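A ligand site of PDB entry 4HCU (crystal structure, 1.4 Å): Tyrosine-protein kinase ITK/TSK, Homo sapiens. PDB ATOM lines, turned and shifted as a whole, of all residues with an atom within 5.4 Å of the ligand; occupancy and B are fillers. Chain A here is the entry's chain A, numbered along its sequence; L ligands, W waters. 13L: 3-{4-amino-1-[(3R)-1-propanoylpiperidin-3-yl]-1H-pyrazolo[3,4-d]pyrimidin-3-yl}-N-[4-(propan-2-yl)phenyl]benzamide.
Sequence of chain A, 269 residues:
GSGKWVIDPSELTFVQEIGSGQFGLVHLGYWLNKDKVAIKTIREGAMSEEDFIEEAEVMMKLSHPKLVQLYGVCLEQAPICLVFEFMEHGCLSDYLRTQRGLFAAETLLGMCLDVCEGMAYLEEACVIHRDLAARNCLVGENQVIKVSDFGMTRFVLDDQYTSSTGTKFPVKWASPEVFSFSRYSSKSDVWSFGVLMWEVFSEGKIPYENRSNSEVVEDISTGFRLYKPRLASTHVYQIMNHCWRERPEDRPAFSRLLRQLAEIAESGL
An oxygen (O38) of the ligand is in hydrogen-bond range of the backbone NH (N) of Cys 91 (2.9 Å).
An oxygen (O37) of the ligand is in hydrogen-bond range of the side-chain amino group (NZ) of Lys 40, 2.8 Å away.
A nitrogen (N36) of the ligand is in hydrogen-bond range of the side-chain carboxylate (OD1) of Asp 149 (2.7 Å).
N of Met 87 is in hydrogen-bond range of N31 of the ligand.
The backbone carbonyl oxygen (O) of Glu 85 is in hydrogen-bond range of a nitrogen (N35) of the ligand (2.7 Å).
The side-chain sulfur (SG) of Cys 91 is bonded to a carbon (C25) of the ligand, at 1.8 Å.
The side-chain sulfur of Cys 91 lies within hydrogen-bond range of the side-chain hydroxyl of Ser 93, 3.6 Å away.
O of Leu 82 is in hydrogen-bond range of N of Lys 40 (2.9 Å).
The backbone NH (N) of Asp 94 lies close to the side-chain sulfur (SG) of Cys 91, 3.7 Å away.
The backbone NH (N) of Ile 18 sits at hydrogen-bond distance from the backbone carbonyl oxygen (O) of Val 26.
O of Gly 19 lies within hydrogen-bond range of N of Val 26, 2.9 Å away.
The backbone carbonyl oxygen (O) of Ala 38 is in hydrogen-bond range of the backbone NH (N) of Phe 84, at 2.8 Å.
CG2 of Ile 18 touches N30 of the ligand, at 3.6 Å.
Ser 20 touches the ligand (O to C20, 3.7 Å).
Val 26 touches the ligand (CG2 to C21, 3.7 Å).
Ala 38 touches the ligand (CB to N35, 3.5 Å).
CD1 of Ile 42 touches C5 of the ligand, at 3.7 Å.
CG of Met 47 touches C27 of the ligand, at 3.8 Å.
CZ of Phe 84 touches C3 of the ligand, at 3.4 Å.
Phe 86 touches the ligand (CA to N31, 3.9 Å).
Gly 90 touches the ligand.
Asp 94 touches the ligand.
Leu 138 touches the ligand (CD1 to C2, 3.6 Å).
Ser 148 touches the ligand.
Met 152 touches the ligand (CE to C7, 3.6 Å).
Phe 155 touches the ligand.
Val 156 touches the ligand (CG2 to C27, 3.8 Å).
Hydrophobic or aromatic side chains that line the ligand: Ile 18, Val 26, Ala 38, Ile 42, Met 47, Phe 84, Phe 86, Met 87, Leu 138, Met 152, Phe 155 and Val 156.
Of the 27 residues printed, 20 come within 4 Å of the ligand.
Along chain A the residues within 4 Å of the ligand span positions 18 to 156.
The nearest printed residue that does not touch the ligand is Phe 23 (4.01 Å).
Water W1 lies within hydrogen-bond range of the side-chain carboxylate (OD2) of Asp 149 and a nitrogen (N36) of the ligand.
Water W6 bridges the side-chain amino group (NZ) of Lys 40 (2.8 Å) and an oxygen (O37) of the ligand (3.3 Å).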
ATOM      1  N   ILE A  18       4.544 -26.086   4.741  1.00  0.00           N
ATOM      2  CA  ILE A  18       4.735 -24.739   5.266  1.00  0.00           C
ATOM      3  C   ILE A  18       6.229 -24.400   5.162  1.00  0.00           C
ATOM      4  O   ILE A  18       6.584 -23.344   4.638  1.00  0.00           O
ATOM      5  CB  ILE A  18       4.191 -24.607   6.704  1.00  0.00           C
ATOM      6  CG1 ILE A  18       2.655 -24.604   6.712  1.00  0.00           C
ATOM      7  CG2 ILE A  18       4.753 -23.334   7.358  1.00  0.00           C
ATOM      8  CD1 ILE A  18       2.021 -24.692   8.119  1.00  0.00           C
ATOM      9  N   GLY A  19       7.084 -25.272   5.696  1.00  0.00           N
ATOM     10  CA  GLY A  19       8.512 -25.051   5.623  1.00  0.00           C
ATOM     11  C   GLY A  19       9.265 -26.071   6.437  1.00  0.00           C
ATOM     12  O   GLY A  19       8.670 -26.857   7.161  1.00  0.00           O
ATOM     13  N   SER A  20      10.577 -26.027   6.329  1.00  0.00           N
ATOM     14  CA  SER A  20      11.469 -26.972   6.985  1.00  0.00           C
ATOM     15  C   SER A  20      11.950 -26.470   8.316  1.00  0.00           C
ATOM     16  O   SER A  20      12.015 -25.258   8.573  1.00  0.00           O
ATOM     17  CB  SER A  20      12.684 -27.213   6.077  1.00  0.00           C
ATOM     18  OG  SER A  20      12.352 -28.036   4.974  1.00  0.00           O
ATOM     19  N   PHE A  23      14.913 -30.404  12.377  1.00  0.00           N
ATOM     20  CA  PHE A  23      14.566 -31.776  12.723  1.00  0.00           C
ATOM     21  C   PHE A  23      13.347 -32.356  12.059  1.00  0.00           C
ATOM     22  O   PHE A  23      12.963 -33.489  12.373  1.00  0.00           O
ATOM     23  CB  PHE A  23      14.467 -31.945  14.256  1.00  0.00           C
ATOM     24  CG  PHE A  23      15.657 -31.377  15.016  1.00  0.00           C
ATOM     25  CD1 PHE A  23      16.930 -31.872  14.789  1.00  0.00           C
ATOM     26  CD2 PHE A  23      15.506 -30.297  15.874  1.00  0.00           C
ATOM     27  CE1 PHE A  23      18.044 -31.315  15.443  1.00  0.00           C
ATOM     28  CE2 PHE A  23      16.609 -29.757  16.539  1.00  0.00           C
ATOM     29  CZ  PHE A  23      17.866 -30.270  16.314  1.00  0.00           C
ATOM     30  N   VAL A  26       7.350 -29.073   8.391  1.00  0.00           N
ATOM     31  CA  VAL A  26       6.072 -28.596   8.882  1.00  0.00           C
ATOM     32  C   VAL A  26       5.121 -28.484   7.697  1.00  0.00           C
ATOM     33  O   VAL A  26       5.460 -27.894   6.657  1.00  0.00           O
ATOM     34  CB  VAL A  26       6.201 -27.232   9.618  1.00  0.00           C
ATOM     35  CG1 VAL A  26       4.857 -26.796  10.224  1.00  0.00           C
ATOM     36  CG2 VAL A  26       7.268 -27.296  10.702  1.00  0.00           C
ATOM     37  N   ALA A  38      -0.951 -26.796  11.927  1.00  0.00           N
ATOM     38  CA  ALA A  38       0.394 -27.014  11.428  1.00  0.00           C
ATOM     39  C   ALA A  38       0.857 -28.350  11.997  1.00  0.00           C
ATOM     40  O   ALA A  38       0.615 -28.629  13.171  1.00  0.00           O
ATOM     41  CB  ALA A  38       1.310 -25.907  11.870  1.00  0.00           C
ATOM     42  N   LYS A  40       4.055 -30.983  12.384  1.00  0.00           N
ATOM     43  CA  LYS A  40       5.475 -31.212  12.289  1.00  0.00           C
ATOM     44  C   LYS A  40       5.756 -32.706  12.277  1.00  0.00           C
ATOM     45  O   LYS A  40       5.348 -33.402  13.212  1.00  0.00           O
ATOM     46  CB  LYS A  40       6.151 -30.573  13.522  1.00  0.00           C
ATOM     47  CG  LYS A  40       7.599 -30.933  13.763  1.00  0.00           C
ATOM     48  CD  LYS A  40       8.473 -30.252  12.769  1.00  0.00           C
ATOM     49  CE  LYS A  40       9.882 -30.129  13.241  1.00  0.00           C
ATOM     50  NZ  LYS A  40      10.078 -28.936  14.111  1.00  0.00           N
ATOM     51  N   ILE A  42       8.703 -35.441  12.818  1.00  0.00           N
ATOM     52  CA  ILE A  42      10.034 -35.375  13.415  1.00  0.00           C
ATOM     53  C   ILE A  42      10.840 -36.585  13.016  1.00  0.00           C
ATOM     54  O   ILE A  42      10.392 -37.702  13.223  1.00  0.00           O
ATOM     55  CB  ILE A  42       9.906 -35.207  14.954  1.00  0.00           C
ATOM     56  CG1 ILE A  42       9.290 -33.823  15.289  1.00  0.00           C
ATOM     57  CG2 ILE A  42      11.271 -35.313  15.659  1.00  0.00           C
ATOM     58  CD1 ILE A  42       8.595 -33.774  16.601  1.00  0.00           C
ATOM     59  N   ALA A  46      15.894 -37.452  16.584  1.00  0.00           N
ATOM     60  CA  ALA A  46      16.058 -36.038  16.871  1.00  0.00           C
ATOM     61  C   ALA A  46      15.536 -35.637  18.232  1.00  0.00           C
ATOM     62  O   ALA A  46      16.034 -34.666  18.802  1.00  0.00           O
ATOM     63  CB  ALA A  46      15.378 -35.211  15.798  1.00  0.00           C
ATOM     64  N   MET A  47      14.544 -36.394  18.745  1.00  0.00           N
ATOM     65  CA  MET A  47      13.835 -36.014  19.956  1.00  0.00           C
ATOM     66  C   MET A  47      13.806 -37.164  20.925  1.00  0.00           C
ATOM     67  O   MET A  47      13.702 -38.322  20.513  1.00  0.00           O
ATOM     68  CB  MET A  47      12.361 -35.649  19.560  1.00  0.00           C
ATOM     69  CG  MET A  47      11.527 -35.138  20.696  1.00  0.00           C
ATOM     70  SD  MET A  47       9.960 -34.495  20.080  1.00  0.00           S
ATOM     71  CE  MET A  47       9.031 -35.924  20.062  1.00  0.00           C
ATOM     72  N   VAL A  68       1.566 -20.249  21.256  1.00  0.00           N
ATOM     73  CA  VAL A  68       1.154 -21.188  20.205  1.00  0.00           C
ATOM     74  C   VAL A  68       0.862 -22.537  20.864  1.00  0.00           C
ATOM     75  O   VAL A  68       1.736 -23.115  21.490  1.00  0.00           O
ATOM     76  CB  VAL A  68       2.237 -21.325  19.123  1.00  0.00           C
ATOM     77  CG1 VAL A  68       1.766 -22.319  18.048  1.00  0.00           C
ATOM     78  CG2 VAL A  68       2.505 -19.967  18.491  1.00  0.00           C
ATOM     79  N   LEU A  82       3.724 -33.854  15.547  1.00  0.00           N
ATOM     80  CA  LEU A  82       3.217 -32.963  16.561  1.00  0.00           C
ATOM     81  C   LEU A  82       2.267 -32.005  15.856  1.00  0.00           C
ATOM     82  O   LEU A  82       2.579 -31.519  14.767  1.00  0.00           O
ATOM     83  CB  LEU A  82       4.316 -32.198  17.261  1.00  0.00           C
ATOM     84  CG  LEU A  82       5.344 -33.031  18.024  1.00  0.00           C
ATOM     85  CD1 LEU A  82       6.222 -32.128  18.898  1.00  0.00           C
ATOM     86  CD2 LEU A  82       4.743 -34.144  18.826  1.00  0.00           C
ATOM     87  N   PHE A  84      -0.007 -28.503  15.926  1.00  0.00           N
ATOM     88  CA  PHE A  84      -0.052 -27.189  16.545  1.00  0.00           C
ATOM     89  C   PHE A  84      -1.083 -26.286  15.930  1.00  0.00           C
ATOM     90  O   PHE A  84      -1.490 -26.427  14.788  1.00  0.00           O
ATOM     91  CB  PHE A  84       1.312 -26.494  16.366  1.00  0.00           C
ATOM     92  CG  PHE A  84       2.478 -27.199  16.987  1.00  0.00           C
ATOM     93  CD1 PHE A  84       2.740 -27.087  18.343  1.00  0.00           C
ATOM     94  CD2 PHE A  84       3.309 -28.010  16.214  1.00  0.00           C
ATOM     95  CE1 PHE A  84       3.800 -27.778  18.924  1.00  0.00           C
ATOM     96  CE2 PHE A  84       4.385 -28.683  16.792  1.00  0.00           C
ATOM     97  CZ  PHE A  84       4.627 -28.558  18.148  1.00  0.00           C
ATOM     98  N   GLU A  85      -1.463 -25.274  16.712  1.00  0.00           N
ATOM     99  CA  GLU A  85      -2.257 -24.166  16.252  1.00  0.00           C
ATOM    100  C   GLU A  85      -1.565 -23.537  15.025  1.00  0.00           C
ATOM    101  O   GLU A  85      -0.351 -23.268  15.077  1.00  0.00           O
ATOM    102  CB  GLU A  85      -2.245 -23.146  17.403  1.00  0.00           C
ATOM    103  CG  GLU A  85      -2.898 -21.839  17.079  1.00  0.00           C
ATOM    104  CD  GLU A  85      -2.879 -20.824  18.201  1.00  0.00           C
ATOM    105  OE1 GLU A  85      -2.343 -21.114  19.298  1.00  0.00           O
ATOM    106  OE2 GLU A  85      -3.465 -19.752  17.986  1.00  0.00           O
ATOM    107  N   PHE A  86      -2.315 -23.317  13.940  1.00  0.00           N
ATOM    108  CA  PHE A  86      -1.776 -22.754  12.720  1.00  0.00           C
ATOM    109  C   PHE A  86      -1.643 -21.249  12.851  1.00  0.00           C
ATOM    110  O   PHE A  86      -2.628 -20.555  13.175  1.00  0.00           O
ATOM    111  CB  PHE A  86      -2.660 -23.125  11.518  1.00  0.00           C
ATOM    112  CG  PHE A  86      -2.251 -22.457  10.232  1.00  0.00           C
ATOM    113  CD1 PHE A  86      -1.001 -22.698   9.667  1.00  0.00           C
ATOM    114  CD2 PHE A  86      -3.089 -21.547   9.606  1.00  0.00           C
ATOM    115  CE1 PHE A  86      -0.603 -22.035   8.487  1.00  0.00           C
ATOM    116  CE2 PHE A  86      -2.718 -20.928   8.416  1.00  0.00           C
ATOM    117  CZ  PHE A  86      -1.480 -21.195   7.852  1.00  0.00           C
ATOM    118  N   MET A  87      -0.436 -20.716  12.539  1.00  0.00           N
ATOM    119  CA  MET A  87      -0.189 -19.268  12.640  1.00  0.00           C
ATOM    120  C   MET A  87      -0.030 -18.750  11.234  1.00  0.00           C
ATOM    121  O   MET A  87       0.988 -19.002  10.573  1.00  0.00           O
ATOM    122  CB  MET A  87       1.057 -19.045  13.475  1.00  0.00           C
ATOM    123  CG  MET A  87       0.949 -19.598  14.889  1.00  0.00           C
ATOM    124  SD  MET A  87      -0.386 -18.888  15.842  1.00  0.00           S
ATOM    125  CE  MET A  87       0.095 -17.168  15.842  1.00  0.00           C
ATOM    126  N   GLU A  88      -1.065 -18.091  10.753  1.00  0.00           N
ATOM    127  CA  GLU A  88      -1.182 -17.710   9.341  1.00  0.00           C
ATOM    128  C   GLU A  88      -0.085 -16.874   8.717  1.00  0.00           C
ATOM    129  O   GLU A  88       0.208 -17.041   7.530  1.00  0.00           O
ATOM    130  CB  GLU A  88      -2.586 -17.160   9.033  1.00  0.00           C
ATOM    131  CG  GLU A  88      -2.920 -15.831   9.677  1.00  0.00           C
ATOM    132  CD  GLU A  88      -4.359 -15.408   9.503  1.00  0.00           C
ATOM    133  OE1 GLU A  88      -5.023 -15.153  10.535  1.00  0.00           O
ATOM    134  OE2 GLU A  88      -4.841 -15.340   8.350  1.00  0.00           O
ATOM    135  N   GLY A  90       3.192 -16.745   9.822  1.00  0.00           N
ATOM    136  CA  GLY A  90       4.511 -17.309  10.030  1.00  0.00           C
ATOM    137  C   GLY A  90       5.424 -16.643  11.023  1.00  0.00           C
ATOM    138  O   GLY A  90       4.970 -15.925  11.922  1.00  0.00           O
ATOM    139  N   CYS A  91       6.740 -16.913  10.909  1.00  0.00           N
ATOM    140  CA  CYS A  91       7.756 -16.437  11.841  1.00  0.00           C
ATOM    141  C   CYS A  91       7.887 -14.941  11.841  1.00  0.00           C
ATOM    142  O   CYS A  91       7.890 -14.294  10.774  1.00  0.00           O
ATOM    143  CB  CYS A  91       9.090 -17.106  11.543  1.00  0.00           C
ATOM    144  SG  CYS A  91       9.696 -16.817   9.862  1.00  0.00           S
ATOM    145  N   SER A  93      10.557 -13.207  12.560  1.00  0.00           N
ATOM    146  CA  SER A  93      11.821 -12.803  11.940  1.00  0.00           C
ATOM    147  C   SER A  93      11.613 -12.454  10.460  1.00  0.00           C
ATOM    148  O   SER A  93      11.916 -11.330  10.019  1.00  0.00           O
ATOM    149  CB  SER A  93      12.837 -13.939  12.106  1.00  0.00           C
ATOM    150  OG  SER A  93      12.232 -15.189  11.796  1.00  0.00           O
ATOM    151  N   ASP A  94      10.984 -13.371   9.688  1.00  0.00           N
ATOM    152  CA  ASP A  94      10.746 -13.097   8.280  1.00  0.00           C
ATOM    153  C   ASP A  94       9.689 -12.042   8.096  1.00  0.00           C
ATOM    154  O   ASP A  94       9.774 -11.284   7.137  1.00  0.00           O
ATOM    155  CB  ASP A  94      10.344 -14.366   7.517  1.00  0.00           C
ATOM    156  CG  ASP A  94      11.450 -15.363   7.240  1.00  0.00           C
ATOM    157  OD1 ASP A  94      12.598 -15.092   7.630  1.00  0.00           O
ATOM    158  OD2 ASP A  94      11.153 -16.436   6.687  1.00  0.00           O
ATOM    159  N   LEU A 138       5.551 -16.330  16.405  1.00  0.00           N
ATOM    160  CA  LEU A 138       4.763 -16.495  15.197  1.00  0.00           C
ATOM    161  C   LEU A 138       3.648 -15.467  15.131  1.00  0.00           C
ATOM    162  O   LEU A 138       3.162 -15.006  16.174  1.00  0.00           O
ATOM    163  CB  LEU A 138       4.238 -17.954  15.117  1.00  0.00           C
ATOM    164  CG  LEU A 138       5.307 -19.078  15.183  1.00  0.00           C
ATOM    165  CD1 LEU A 138       4.640 -20.450  15.049  1.00  0.00           C
ATOM    166  CD2 LEU A 138       6.386 -18.893  14.130  1.00  0.00           C
ATOM    167  N   SER A 148       6.198 -19.514  20.587  1.00  0.00           N
ATOM    168  CA  SER A 148       6.180 -20.962  20.379  1.00  0.00           C
ATOM    169  C   SER A 148       7.436 -21.598  20.913  1.00  0.00           C
ATOM    170  O   SER A 148       8.471 -20.939  21.112  1.00  0.00           O
ATOM    171  CB  SER A 148       6.021 -21.313  18.911  1.00  0.00           C
ATOM    172  OG  SER A 148       7.215 -21.113  18.192  1.00  0.00           O
ATOM    173  N   ASP A 149       7.386 -22.922  21.059  1.00  0.00           N
ATOM    174  CA  ASP A 149       8.556 -23.732  21.353  1.00  0.00           C
ATOM    175  C   ASP A 149       9.102 -23.591  22.743  1.00  0.00           C
ATOM    176  O   ASP A 149      10.198 -24.061  23.024  1.00  0.00           O
ATOM    177  CB  ASP A 149       9.649 -23.678  20.252  1.00  0.00           C
ATOM    178  CG  ASP A 149       9.283 -24.492  19.024  1.00  0.00           C
ATOM    179  OD1 ASP A 149       8.365 -25.318  19.132  1.00  0.00           O
ATOM    180  OD2 ASP A 149       9.924 -24.286  17.984  1.00  0.00           O
ATOM    181  N   MET A 152      10.963 -26.652  24.516  1.00  0.00           N
ATOM    182  CA  MET A 152      11.249 -27.729  23.553  1.00  0.00           C
ATOM    183  C   MET A 152      12.680 -28.166  23.514  1.00  0.00           C
ATOM    184  O   MET A 152      12.925 -29.334  23.159  1.00  0.00           O
ATOM    185  CB  MET A 152      10.710 -27.387  22.154  1.00  0.00           C
ATOM    186  CG  MET A 152       9.167 -27.306  22.115  1.00  0.00           C
ATOM    187  SD  MET A 152       8.360 -28.891  22.521  1.00  0.00           S
ATOM    188  CE  MET A 152       8.524 -29.764  20.990  1.00  0.00           C
ATOM    189  N   PHE A 155      13.961 -31.617  24.885  1.00  0.00           N
ATOM    190  CA  PHE A 155      13.786 -32.898  24.214  1.00  0.00           C
ATOM    191  C   PHE A 155      14.720 -33.076  23.020  1.00  0.00           C
ATOM    192  O   PHE A 155      14.684 -34.150  22.398  1.00  0.00           O
ATOM    193  CB  PHE A 155      12.325 -33.020  23.728  1.00  0.00           C
ATOM    194  CG  PHE A 155      11.343 -32.700  24.830  1.00  0.00           C
ATOM    195  CD1 PHE A 155      11.182 -33.557  25.908  1.00  0.00           C
ATOM    196  CD2 PHE A 155      10.655 -31.497  24.832  1.00  0.00           C
ATOM    197  CE1 PHE A 155      10.294 -33.235  26.958  1.00  0.00           C
ATOM    198  CE2 PHE A 155       9.761 -31.177  25.873  1.00  0.00           C
ATOM    199  CZ  PHE A 155       9.594 -32.054  26.911  1.00  0.00           C
ATOM    200  N   VAL A 156      15.545 -32.079  22.675  1.00  0.00           N
ATOM    201  CA  VAL A 156      16.444 -32.188  21.516  1.00  0.00           C
ATOM    202  C   VAL A 156      17.622 -33.099  21.861  1.00  0.00           C
ATOM    203  O   VAL A 156      18.268 -32.900  22.890  1.00  0.00           O
ATOM    204  CB  VAL A 156      16.933 -30.762  21.125  1.00  0.00           C
ATOM    205  CG1 VAL A 156      18.061 -30.819  20.083  1.00  0.00           C
ATOM    206  CG2 VAL A 156      15.774 -29.921  20.584  1.00  0.00           C
HETATM  207  C4  13L L   1      11.411 -28.769  18.475  1.00  0.00           C
HETATM  208  C7  13L L   1       9.037 -29.655  17.408  1.00  0.00           C
HETATM  209  C6  13L L   1      10.421 -27.858  18.162  1.00  0.00           C
HETATM  210  C9  13L L   1       2.658 -21.802  11.043  1.00  0.00           C
HETATM  211  C13 13L L   1      11.225 -30.125  18.267  1.00  0.00           C
HETATM  212  C20 13L L   1       9.027 -23.128   9.165  1.00  0.00           C
HETATM  213  C21 13L L   1       7.901 -23.685  10.039  1.00  0.00           C
HETATM  214  C8  13L L   1       6.331 -25.544  14.792  1.00  0.00           C
HETATM  215  C18 13L L   1       7.520 -27.243  16.146  1.00  0.00           C
HETATM  216  C16 13L L   1       4.642 -22.670  11.539  1.00  0.00           C
HETATM  217  C19 13L L   1       8.324 -19.779   9.243  1.00  0.00           C
HETATM  218  C26 13L L   1      12.554 -32.237  17.763  1.00  0.00           C
HETATM  219  C1  13L L   1       5.117 -24.503  17.046  1.00  0.00           C
HETATM  220  C2  13L L   1       4.882 -23.950  15.805  1.00  0.00           C
HETATM  221  C3  13L L   1       5.980 -25.570  17.181  1.00  0.00           C
HETATM  222  C5  13L L   1      10.033 -30.564  17.729  1.00  0.00           C
HETATM  223  C10 13L L   1       4.171 -23.211  12.722  1.00  0.00           C
HETATM  224  C11 13L L   1       5.472 -24.464  14.651  1.00  0.00           C
HETATM  225  C12 13L L   1       6.576 -26.104  16.040  1.00  0.00           C
HETATM  226  C14 13L L   1       9.233 -28.306  17.623  1.00  0.00           C
HETATM  227  C15 13L L   1       5.307 -23.841  13.336  1.00  0.00           C
HETATM  228  C17 13L L   1       2.818 -23.007  13.008  1.00  0.00           C
HETATM  229  C22 13L L   1       9.622 -21.872   9.799  1.00  0.00           C
HETATM  230  C23 13L L   1       7.559 -21.340  10.964  1.00  0.00           C
HETATM  231  C24 13L L   1       6.888 -22.605  10.420  1.00  0.00           C
HETATM  232  C25 13L L   1      10.375 -18.381   9.211  1.00  0.00           C
HETATM  233  C27 13L L   1      12.313 -31.427  20.118  1.00  0.00           C
HETATM  234  C28 13L L   1       9.481 -19.300   8.412  1.00  0.00           C
HETATM  235  C29 13L L   1      12.377 -31.030  18.652  1.00  0.00           C
HETATM  236  N30 13L L   1       3.933 -21.972  10.643  1.00  0.00           N
HETATM  237  N31 13L L   1       2.070 -22.286  12.147  1.00  0.00           N
HETATM  238  N32 13L L   1       6.375 -23.730  12.537  1.00  0.00           N
HETATM  239  N33 13L L   1       5.949 -23.045  11.451  1.00  0.00           N
HETATM  240  N34 13L L   1       8.575 -20.889  10.038  1.00  0.00           N
HETATM  241  N35 13L L   1       2.223 -23.500  14.168  1.00  0.00           N
HETATM  242  N36 13L L   1       8.212 -27.344  17.321  1.00  0.00           N
HETATM  243  O37 13L L   1       7.666 -28.034  15.225  1.00  0.00           O
HETATM  244  O38 13L L   1       7.250 -19.180   9.180  1.00  0.00           O
HETATM  245  O   HOH W   1       9.694 -24.880  15.408  1.00  0.00           O
HETATM  246  O   HOH W   2       7.031 -16.884   6.672  1.00  0.00           O
HETATM  247  O   HOH W   3       4.491 -20.202   8.389  1.00  0.00           O
HETATM  248  O   HOH W   4       6.245 -26.308  20.533  1.00  0.00           O
HETATM  249  O   HOH W   5       8.048 -21.332   6.056  1.00  0.00           O
HETATM  250  O   HOH W   6       9.691 -26.320  13.190  1.00  0.00           O
